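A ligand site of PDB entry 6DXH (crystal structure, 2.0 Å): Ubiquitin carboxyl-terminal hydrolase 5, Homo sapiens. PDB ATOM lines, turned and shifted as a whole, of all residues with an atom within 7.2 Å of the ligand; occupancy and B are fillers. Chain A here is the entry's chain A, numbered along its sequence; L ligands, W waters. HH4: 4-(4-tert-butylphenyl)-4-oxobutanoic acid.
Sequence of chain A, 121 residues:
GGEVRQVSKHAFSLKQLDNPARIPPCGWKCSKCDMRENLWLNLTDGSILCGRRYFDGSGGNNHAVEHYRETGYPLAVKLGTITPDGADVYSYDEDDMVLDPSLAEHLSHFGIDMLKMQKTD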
ATOM      1  N   ARG A   5     -14.871 -15.225  -7.342  1.00  0.00           N
ATOM      2  CA  ARG A   5     -14.884 -15.947  -8.636  1.00  0.00           C
ATOM      3  C   ARG A   5     -14.718 -17.442  -8.362  1.00  0.00           C
ATOM      4  O   ARG A   5     -14.061 -17.838  -7.439  1.00  0.00           O
ATOM      5  CB  ARG A   5     -13.771 -15.416  -9.552  1.00  0.00           C
ATOM      6  CG  ARG A   5     -14.059 -14.041 -10.125  1.00  0.00           C
ATOM      7  CD  ARG A   5     -12.853 -13.418 -10.809  1.00  0.00           C
ATOM      8  NE  ARG A   5     -13.090 -11.984 -11.039  1.00  0.00           N
ATOM      9  CZ  ARG A   5     -12.295 -11.178 -11.740  1.00  0.00           C
ATOM     10  NH1 ARG A   5     -11.301 -11.671 -12.451  1.00  0.00           N
ATOM     11  NH2 ARG A   5     -12.562  -9.877 -11.773  1.00  0.00           N
ATOM     12  N   ASN A  38      -9.417  -3.823 -24.765  1.00  0.00           N
ATOM     13  CA  ASN A  38     -10.463  -4.865 -24.495  1.00  0.00           C
ATOM     14  C   ASN A  38     -10.293  -6.048 -25.459  1.00  0.00           C
ATOM     15  O   ASN A  38     -11.272  -6.518 -26.044  1.00  0.00           O
ATOM     16  CB  ASN A  38     -11.904  -4.366 -24.641  1.00  0.00           C
ATOM     17  CG  ASN A  38     -12.341  -3.347 -23.610  1.00  0.00           C
ATOM     18  OD1 ASN A  38     -13.279  -2.573 -23.879  1.00  0.00           O
ATOM     19  ND2 ASN A  38     -11.681  -3.326 -22.456  1.00  0.00           N
ATOM     20  N   TRP A  40      -9.264 -10.103 -26.125  1.00  0.00           N
ATOM     21  CA  TRP A  40      -9.481 -11.338 -25.467  1.00  0.00           C
ATOM     22  C   TRP A  40      -8.857 -12.504 -26.243  1.00  0.00           C
ATOM     23  O   TRP A  40      -9.104 -12.681 -27.467  1.00  0.00           O
ATOM     24  CB  TRP A  40     -10.980 -11.536 -25.319  1.00  0.00           C
ATOM     25  CG  TRP A  40     -11.605 -10.533 -24.430  1.00  0.00           C
ATOM     26  CD1 TRP A  40     -12.106  -9.327 -24.797  1.00  0.00           C
ATOM     27  CD2 TRP A  40     -11.805 -10.658 -23.021  1.00  0.00           C
ATOM     28  NE1 TRP A  40     -12.623  -8.694 -23.691  1.00  0.00           N
ATOM     29  CE2 TRP A  40     -12.458  -9.481 -22.593  1.00  0.00           C
ATOM     30  CE3 TRP A  40     -11.507 -11.642 -22.080  1.00  0.00           C
ATOM     31  CZ2 TRP A  40     -12.805  -9.256 -21.277  1.00  0.00           C
ATOM     32  CZ3 TRP A  40     -11.862 -11.422 -20.765  1.00  0.00           C
ATOM     33  CH2 TRP A  40     -12.513 -10.246 -20.367  1.00  0.00           C
ATOM     34  N   LEU A  49      -8.984 -11.264 -30.278  1.00  0.00           N
ATOM     35  CA  LEU A  49     -10.149 -10.576 -30.900  1.00  0.00           C
ATOM     36  C   LEU A  49     -10.736  -9.613 -29.889  1.00  0.00           C
ATOM     37  O   LEU A  49     -10.613  -9.864 -28.680  1.00  0.00           O
ATOM     38  CB  LEU A  49     -11.211 -11.591 -31.347  1.00  0.00           C
ATOM     39  CG  LEU A  49     -10.748 -12.616 -32.392  1.00  0.00           C
ATOM     40  CD1 LEU A  49     -11.819 -13.697 -32.565  1.00  0.00           C
ATOM     41  CD2 LEU A  49     -10.442 -11.936 -33.741  1.00  0.00           C
ATOM     42  N   CYS A  50     -11.382  -8.534 -30.378  1.00  0.00           N
ATOM     43  CA  CYS A  50     -11.833  -7.431 -29.532  1.00  0.00           C
ATOM     44  C   CYS A  50     -13.132  -7.753 -28.772  1.00  0.00           C
ATOM     45  O   CYS A  50     -13.966  -8.599 -29.177  1.00  0.00           O
ATOM     46  CB  CYS A  50     -11.933  -6.173 -30.402  1.00  0.00           C
ATOM     47  SG  CYS A  50     -13.111  -6.304 -31.772  1.00  0.00           S
ATOM     48  N   GLY A  51     -13.319  -7.046 -27.638  1.00  0.00           N
ATOM     49  CA  GLY A  51     -14.473  -7.171 -26.759  1.00  0.00           C
ATOM     50  C   GLY A  51     -15.765  -6.546 -27.301  1.00  0.00           C
ATOM     51  O   GLY A  51     -15.796  -5.943 -28.377  1.00  0.00           O
ATOM     52  N   ARG A  52     -16.846  -6.745 -26.552  1.00  0.00           N
ATOM     53  CA  ARG A  52     -18.178  -6.323 -26.914  1.00  0.00           C
ATOM     54  C   ARG A  52     -18.201  -4.809 -27.020  1.00  0.00           C
ATOM     55  O   ARG A  52     -17.468  -4.117 -26.313  1.00  0.00           O
ATOM     56  CB  ARG A  52     -19.217  -6.783 -25.883  1.00  0.00           C
ATOM     57  CG  ARG A  52     -19.465  -8.281 -25.891  1.00  0.00           C
ATOM     58  CD  ARG A  52     -20.120  -8.744 -24.608  1.00  0.00           C
ATOM     59  NE  ARG A  52     -21.265  -9.599 -24.882  1.00  0.00           N
ATOM     60  CZ  ARG A  52     -21.436 -10.847 -24.449  1.00  0.00           C
ATOM     61  NH1 ARG A  52     -20.586 -11.403 -23.597  1.00  0.00           N
ATOM     62  NH2 ARG A  52     -22.492 -11.533 -24.864  1.00  0.00           N
ATOM     63  N   ARG A  53     -18.960  -4.315 -28.012  1.00  0.00           N
ATOM     64  CA  ARG A  53     -19.161  -2.888 -28.237  1.00  0.00           C
ATOM     65  C   ARG A  53     -20.019  -2.334 -27.088  1.00  0.00           C
ATOM     66  O   ARG A  53     -20.948  -2.988 -26.646  1.00  0.00           O
ATOM     67  CB  ARG A  53     -19.867  -2.667 -29.574  1.00  0.00           C
ATOM     68  CG  ARG A  53     -20.136  -1.206 -29.908  1.00  0.00           C
ATOM     69  CD  ARG A  53     -20.664  -1.118 -31.317  1.00  0.00           C
ATOM     70  NE  ARG A  53     -19.591  -1.369 -32.275  1.00  0.00           N
ATOM     71  CZ  ARG A  53     -19.743  -2.019 -33.423  1.00  0.00           C
ATOM     72  NH1 ARG A  53     -20.942  -2.415 -33.811  1.00  0.00           N
ATOM     73  NH2 ARG A  53     -18.687  -2.270 -34.182  1.00  0.00           N
ATOM     74  N   TYR A  54     -19.649  -1.161 -26.574  1.00  0.00           N
ATOM     75  CA  TYR A  54     -20.409  -0.531 -25.476  1.00  0.00           C
ATOM     76  C   TYR A  54     -21.699   0.092 -26.051  1.00  0.00           C
ATOM     77  O   TYR A  54     -21.786   0.315 -27.260  1.00  0.00           O
ATOM     78  CB  TYR A  54     -19.515   0.493 -24.761  1.00  0.00           C
ATOM     79  CG  TYR A  54     -18.381  -0.097 -23.945  1.00  0.00           C
ATOM     80  CD1 TYR A  54     -18.530  -1.292 -23.232  1.00  0.00           C
ATOM     81  CD2 TYR A  54     -17.160   0.544 -23.869  1.00  0.00           C
ATOM     82  CE1 TYR A  54     -17.495  -1.815 -22.452  1.00  0.00           C
ATOM     83  CE2 TYR A  54     -16.114   0.024 -23.120  1.00  0.00           C
ATOM     84  CZ  TYR A  54     -16.279  -1.159 -22.433  1.00  0.00           C
ATOM     85  OH  TYR A  54     -15.243  -1.638 -21.683  1.00  0.00           O
ATOM     86  N   ASN A  62     -17.094  -6.436 -31.146  1.00  0.00           N
ATOM     87  CA  ASN A  62     -17.753  -7.723 -30.883  1.00  0.00           C
ATOM     88  C   ASN A  62     -17.039  -8.921 -31.521  1.00  0.00           C
ATOM     89  O   ASN A  62     -17.678  -9.929 -31.686  1.00  0.00           O
ATOM     90  CB  ASN A  62     -19.191  -7.711 -31.403  1.00  0.00           C
ATOM     91  CG  ASN A  62     -19.955  -6.567 -30.817  1.00  0.00           C
ATOM     92  OD1 ASN A  62     -19.964  -6.411 -29.603  1.00  0.00           O
ATOM     93  ND2 ASN A  62     -20.510  -5.724 -31.676  1.00  0.00           N
ATOM     94  N   HIS A  63     -15.771  -8.830 -31.881  1.00  0.00           N
ATOM     95  CA  HIS A  63     -15.160  -9.971 -32.649  1.00  0.00           C
ATOM     96  C   HIS A  63     -14.971 -11.228 -31.787  1.00  0.00           C
ATOM     97  O   HIS A  63     -15.233 -12.327 -32.293  1.00  0.00           O
ATOM     98  CB  HIS A  63     -13.909  -9.505 -33.388  1.00  0.00           C
ATOM     99  CG  HIS A  63     -14.265  -8.598 -34.510  1.00  0.00           C
ATOM    100  ND1 HIS A  63     -13.540  -7.467 -34.798  1.00  0.00           N
ATOM    101  CD2 HIS A  63     -15.294  -8.652 -35.398  1.00  0.00           C
ATOM    102  CE1 HIS A  63     -14.065  -6.901 -35.877  1.00  0.00           C
ATOM    103  NE2 HIS A  63     -15.179  -7.587 -36.235  1.00  0.00           N
ATOM    104  N   ALA A  64     -14.668 -11.077 -30.503  1.00  0.00           N
ATOM    105  CA  ALA A  64     -14.463 -12.230 -29.616  1.00  0.00           C
ATOM    106  C   ALA A  64     -15.789 -12.950 -29.339  1.00  0.00           C
ATOM    107  O   ALA A  64     -15.883 -14.170 -29.364  1.00  0.00           O
ATOM    108  CB  ALA A  64     -13.843 -11.749 -28.329  1.00  0.00           C
ATOM    109  N   VAL A  65     -16.845 -12.168 -29.107  1.00  0.00           N
ATOM    110  CA  VAL A  65     -18.112 -12.763 -28.763  1.00  0.00           C
ATOM    111  C   VAL A  65     -18.686 -13.431 -30.009  1.00  0.00           C
ATOM    112  O   VAL A  65     -19.214 -14.523 -29.906  1.00  0.00           O
ATOM    113  CB  VAL A  65     -19.065 -11.757 -28.110  1.00  0.00           C
ATOM    114  CG1 VAL A  65     -19.459 -10.625 -29.046  1.00  0.00           C
ATOM    115  CG2 VAL A  65     -20.307 -12.459 -27.567  1.00  0.00           C
ATOM    116  N   GLU A  66     -18.542 -12.794 -31.176  1.00  0.00           N
ATOM    117  CA  GLU A  66     -19.005 -13.419 -32.422  1.00  0.00           C
ATOM    118  C   GLU A  66     -18.269 -14.734 -32.604  1.00  0.00           C
ATOM    119  O   GLU A  66     -18.882 -15.716 -32.962  1.00  0.00           O
ATOM    120  CB  GLU A  66     -18.817 -12.503 -33.636  1.00  0.00           C
ATOM    121  CG  GLU A  66     -19.737 -11.304 -33.601  1.00  0.00           C
ATOM    122  CD  GLU A  66     -19.516 -10.238 -34.645  1.00  0.00           C
ATOM    123  OE1 GLU A  66     -18.575 -10.365 -35.465  1.00  0.00           O
ATOM    124  OE2 GLU A  66     -20.241  -9.257 -34.602  1.00  0.00           O
ATOM    125  N   ALA A  76     -11.943 -17.142 -22.331  1.00  0.00           N
ATOM    126  CA  ALA A  76     -11.043 -16.152 -22.859  1.00  0.00           C
ATOM    127  C   ALA A  76     -10.399 -15.347 -21.720  1.00  0.00           C
ATOM    128  O   ALA A  76     -11.021 -15.087 -20.700  1.00  0.00           O
ATOM    129  CB  ALA A  76     -11.812 -15.254 -23.787  1.00  0.00           C
ATOM    130  N   LYS A  78      -8.255 -11.741 -20.795  1.00  0.00           N
ATOM    131  CA  LYS A  78      -8.167 -10.390 -21.245  1.00  0.00           C
ATOM    132  C   LYS A  78      -6.690  -9.994 -21.278  1.00  0.00           C
ATOM    133  O   LYS A  78      -6.014 -10.025 -20.232  1.00  0.00           O
ATOM    134  CB  LYS A  78      -8.918  -9.474 -20.314  1.00  0.00           C
ATOM    135  CG  LYS A  78      -9.050  -8.035 -20.802  1.00  0.00           C
ATOM    136  CD  LYS A  78      -9.803  -7.236 -19.755  1.00  0.00           C
ATOM    137  CE  LYS A  78     -10.234  -5.869 -20.233  1.00  0.00           C
ATOM    138  NZ  LYS A  78     -11.253  -5.318 -19.297  1.00  0.00           N
ATOM    139  N   TYR A  90     -12.795 -14.677 -18.523  1.00  0.00           N
ATOM    140  CA  TYR A  90     -14.232 -14.663 -18.710  1.00  0.00           C
ATOM    141  C   TYR A  90     -14.687 -15.952 -19.360  1.00  0.00           C
ATOM    142  O   TYR A  90     -13.989 -16.465 -20.255  1.00  0.00           O
ATOM    143  CB  TYR A  90     -14.661 -13.442 -19.537  1.00  0.00           C
ATOM    144  CG  TYR A  90     -16.139 -13.385 -19.813  1.00  0.00           C
ATOM    145  CD1 TYR A  90     -17.069 -13.063 -18.819  1.00  0.00           C
ATOM    146  CD2 TYR A  90     -16.628 -13.682 -21.075  1.00  0.00           C
ATOM    147  CE1 TYR A  90     -18.427 -13.025 -19.102  1.00  0.00           C
ATOM    148  CE2 TYR A  90     -17.976 -13.661 -21.363  1.00  0.00           C
ATOM    149  CZ  TYR A  90     -18.890 -13.328 -20.379  1.00  0.00           C
ATOM    150  OH  TYR A  90     -20.197 -13.342 -20.752  1.00  0.00           O
ATOM    151  N   SER A  91     -15.832 -16.460 -18.912  1.00  0.00           N
ATOM    152  CA  SER A  91     -16.539 -17.622 -19.514  1.00  0.00           C
ATOM    153  C   SER A  91     -17.809 -17.124 -20.216  1.00  0.00           C
ATOM    154  O   SER A  91     -18.668 -16.496 -19.576  1.00  0.00           O
ATOM    155  CB  SER A  91     -16.870 -18.644 -18.490  1.00  0.00           C
ATOM    156  OG  SER A  91     -17.571 -19.731 -19.063  1.00  0.00           O
ATOM    157  N   TYR A  92     -17.864 -17.326 -21.538  1.00  0.00           N
ATOM    158  CA  TYR A  92     -18.987 -16.916 -22.391  1.00  0.00           C
ATOM    159  C   TYR A  92     -20.174 -17.810 -22.038  1.00  0.00           C
ATOM    160  O   TYR A  92     -21.318 -17.427 -22.045  1.00  0.00           O
ATOM    161  CB  TYR A  92     -18.621 -17.081 -23.870  1.00  0.00           C
ATOM    162  CG  TYR A  92     -17.767 -15.969 -24.456  1.00  0.00           C
ATOM    163  CD1 TYR A  92     -18.314 -14.717 -24.744  1.00  0.00           C
ATOM    164  CD2 TYR A  92     -16.418 -16.143 -24.685  1.00  0.00           C
ATOM    165  CE1 TYR A  92     -17.536 -13.705 -25.276  1.00  0.00           C
ATOM    166  CE2 TYR A  92     -15.626 -15.136 -25.219  1.00  0.00           C
ATOM    167  CZ  TYR A  92     -16.187 -13.901 -25.510  1.00  0.00           C
ATOM    168  OH  TYR A  92     -15.411 -12.910 -26.016  1.00  0.00           O
ATOM    169  N   ASP A  95     -21.203 -17.133 -18.465  1.00  0.00           N
ATOM    170  CA  ASP A  95     -21.448 -15.702 -18.394  1.00  0.00           C
ATOM    171  C   ASP A  95     -20.955 -15.121 -17.070  1.00  0.00           C
ATOM    172  O   ASP A  95     -21.673 -14.371 -16.412  1.00  0.00           O
ATOM    173  CB  ASP A  95     -22.916 -15.345 -18.688  1.00  0.00           C
ATOM    174  CG  ASP A  95     -23.167 -13.842 -18.827  1.00  0.00           C
ATOM    175  OD1 ASP A  95     -22.164 -13.038 -18.957  1.00  0.00           O
ATOM    176  OD2 ASP A  95     -24.349 -13.454 -18.756  1.00  0.00           O
ATOM    177  N   ASP A  96     -19.676 -15.342 -16.733  1.00  0.00           N
ATOM    178  CA  ASP A  96     -19.065 -14.746 -15.530  1.00  0.00           C
ATOM    179  C   ASP A  96     -17.559 -14.630 -15.700  1.00  0.00           C
ATOM    180  O   ASP A  96     -16.969 -15.336 -16.520  1.00  0.00           O
ATOM    181  CB  ASP A  96     -19.279 -15.632 -14.306  1.00  0.00           C
ATOM    182  CG  ASP A  96     -20.414 -15.180 -13.425  1.00  0.00           C
ATOM    183  OD1 ASP A  96     -20.342 -14.006 -12.985  1.00  0.00           O
ATOM    184  OD2 ASP A  96     -21.347 -15.992 -13.231  1.00  0.00           O
ATOM    185  N   MET A  97     -16.948 -13.809 -14.854  1.00  0.00           N
ATOM    186  CA  MET A  97     -15.544 -13.915 -14.614  1.00  0.00           C
ATOM    187  C   MET A  97     -15.324 -15.189 -13.801  1.00  0.00           C
ATOM    188  O   MET A  97     -16.091 -15.470 -12.876  1.00  0.00           O
ATOM    189  CB  MET A  97     -14.992 -12.719 -13.842  1.00  0.00           C
ATOM    190  CG  MET A  97     -15.278 -11.388 -14.499  1.00  0.00           C
ATOM    191  SD  MET A  97     -14.731 -11.342 -16.221  1.00  0.00           S
ATOM    192  CE  MET A  97     -12.974 -11.098 -16.019  1.00  0.00           C
HETATM  193  C4  HH4 L   1     -18.661  -9.351 -17.906  1.00  0.00           C
HETATM  194  C2  HH4 L   1     -18.186  -8.636 -15.498  1.00  0.00           C
HETATM  195  C3  HH4 L   1     -20.498  -8.569 -16.405  1.00  0.00           C
HETATM  196  C1  HH4 L   1     -19.164  -9.314 -16.458  1.00  0.00           C
HETATM  197  C7  HH4 L   1     -17.769  -9.822 -20.521  1.00  0.00           C
HETATM  198  C6  HH4 L   1     -19.107  -9.974 -20.190  1.00  0.00           C
HETATM  199  C8  HH4 L   1     -16.887  -9.359 -19.545  1.00  0.00           C
HETATM  200  C12 HH4 L   1     -15.633 -10.671 -23.666  1.00  0.00           C
HETATM  201  C13 HH4 L   1     -16.148  -9.759 -24.760  1.00  0.00           C
HETATM  202  C9  HH4 L   1     -17.330  -9.116 -18.256  1.00  0.00           C
HETATM  203  C5  HH4 L   1     -19.550  -9.755 -18.898  1.00  0.00           C
HETATM  204  C11 HH4 L   1     -15.895 -10.143 -22.260  1.00  0.00           C
HETATM  205  O1  HH4 L   1     -16.339  -8.513 -24.525  1.00  0.00           O
HETATM  206  O2  HH4 L   1     -18.180 -10.546 -22.720  1.00  0.00           O
HETATM  207  C10 HH4 L   1     -17.352 -10.213 -21.897  1.00  0.00           C
HETATM  208  O   HH4 L   1     -16.349 -10.311 -25.857  1.00  0.00           O
HETATM  209  C   HH4 L   1     -19.439 -10.762 -15.994  1.00  0.00           C
HETATM  210  O   HOH W   1     -14.714  -6.667 -23.307  1.00  0.00           O
HETATM  211  O   HOH W   2     -16.507  -9.437 -28.366  1.00  0.00           O
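NH1 of Arg 52 lies within hydrogen-bond range of OH of Tyr 90 (3.5 Å). N of Gly 51 lies within hydrogen-bond range of O of Asn 38 (2.6 Å). The backbone NH of Asn 62 lies within hydrogen-bond range of the backbone carbonyl oxygen of Gly 51. The side-chain carboxylate (OD1) of Asp 95 sits at hydrogen-bond distance from the side-chain hydroxyl (OH) of Tyr 90, 2.7 Å away. The backbone NH (N) of Tyr 90 is in hydrogen-bond range of the backbone carbonyl oxygen (O) of Ala 76 (2.8 Å). NE1 of Trp 40 sits close to O of Asn 38, at 3.5 Å. N of Trp 40 sits at hydrogen-bond distance from O of Leu 49 (2.9 Å). The backbone NH (N) of Ala 64 is in hydrogen-bond range of the backbone carbonyl oxygen (O) of Cys 50, 2.9 Å away.
The backbone NH (N) of Arg 52 lies within hydrogen-bond range of an oxygen (O1) of the ligand, at 2.7 Å. The guanidinium group (NH1) of Arg 52 lies within hydrogen-bond range of an oxygen (O2) of the ligand (2.7 Å). O of the ligand lies within hydrogen-bond range of OH of Tyr 92.
Water W1 lies within hydrogen-bond range of O1 of the ligand (2.7 Å) and NE1 of Trp 40 (2.9 Å).
Trp 40 touches the ligand. CA of Gly 51 touches O1 of the ligand, at 3.2 Å. Ala 64 touches the ligand. N of Val 65 touches O of the ligand (3.8 Å). CE1 of Tyr 90 touches C6 of the ligand, at 3.3 Å. SD of Met 97 touches C9 of the ligand, at 3.98 Å. Hydrophobic or aromatic side chains within 4 Å of the ligand: Trp 40, Ala 64, Val 65, Tyr 90, Tyr 92 and Met 97. Within 4 Å of the ligand: Trp 40, Gly 51, Arg 52, Ala 64, Val 65, Tyr 90, Tyr 92 and Met 97. The nearest printed residue that does not touch the ligand is Asp 96 (4.03 Å).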
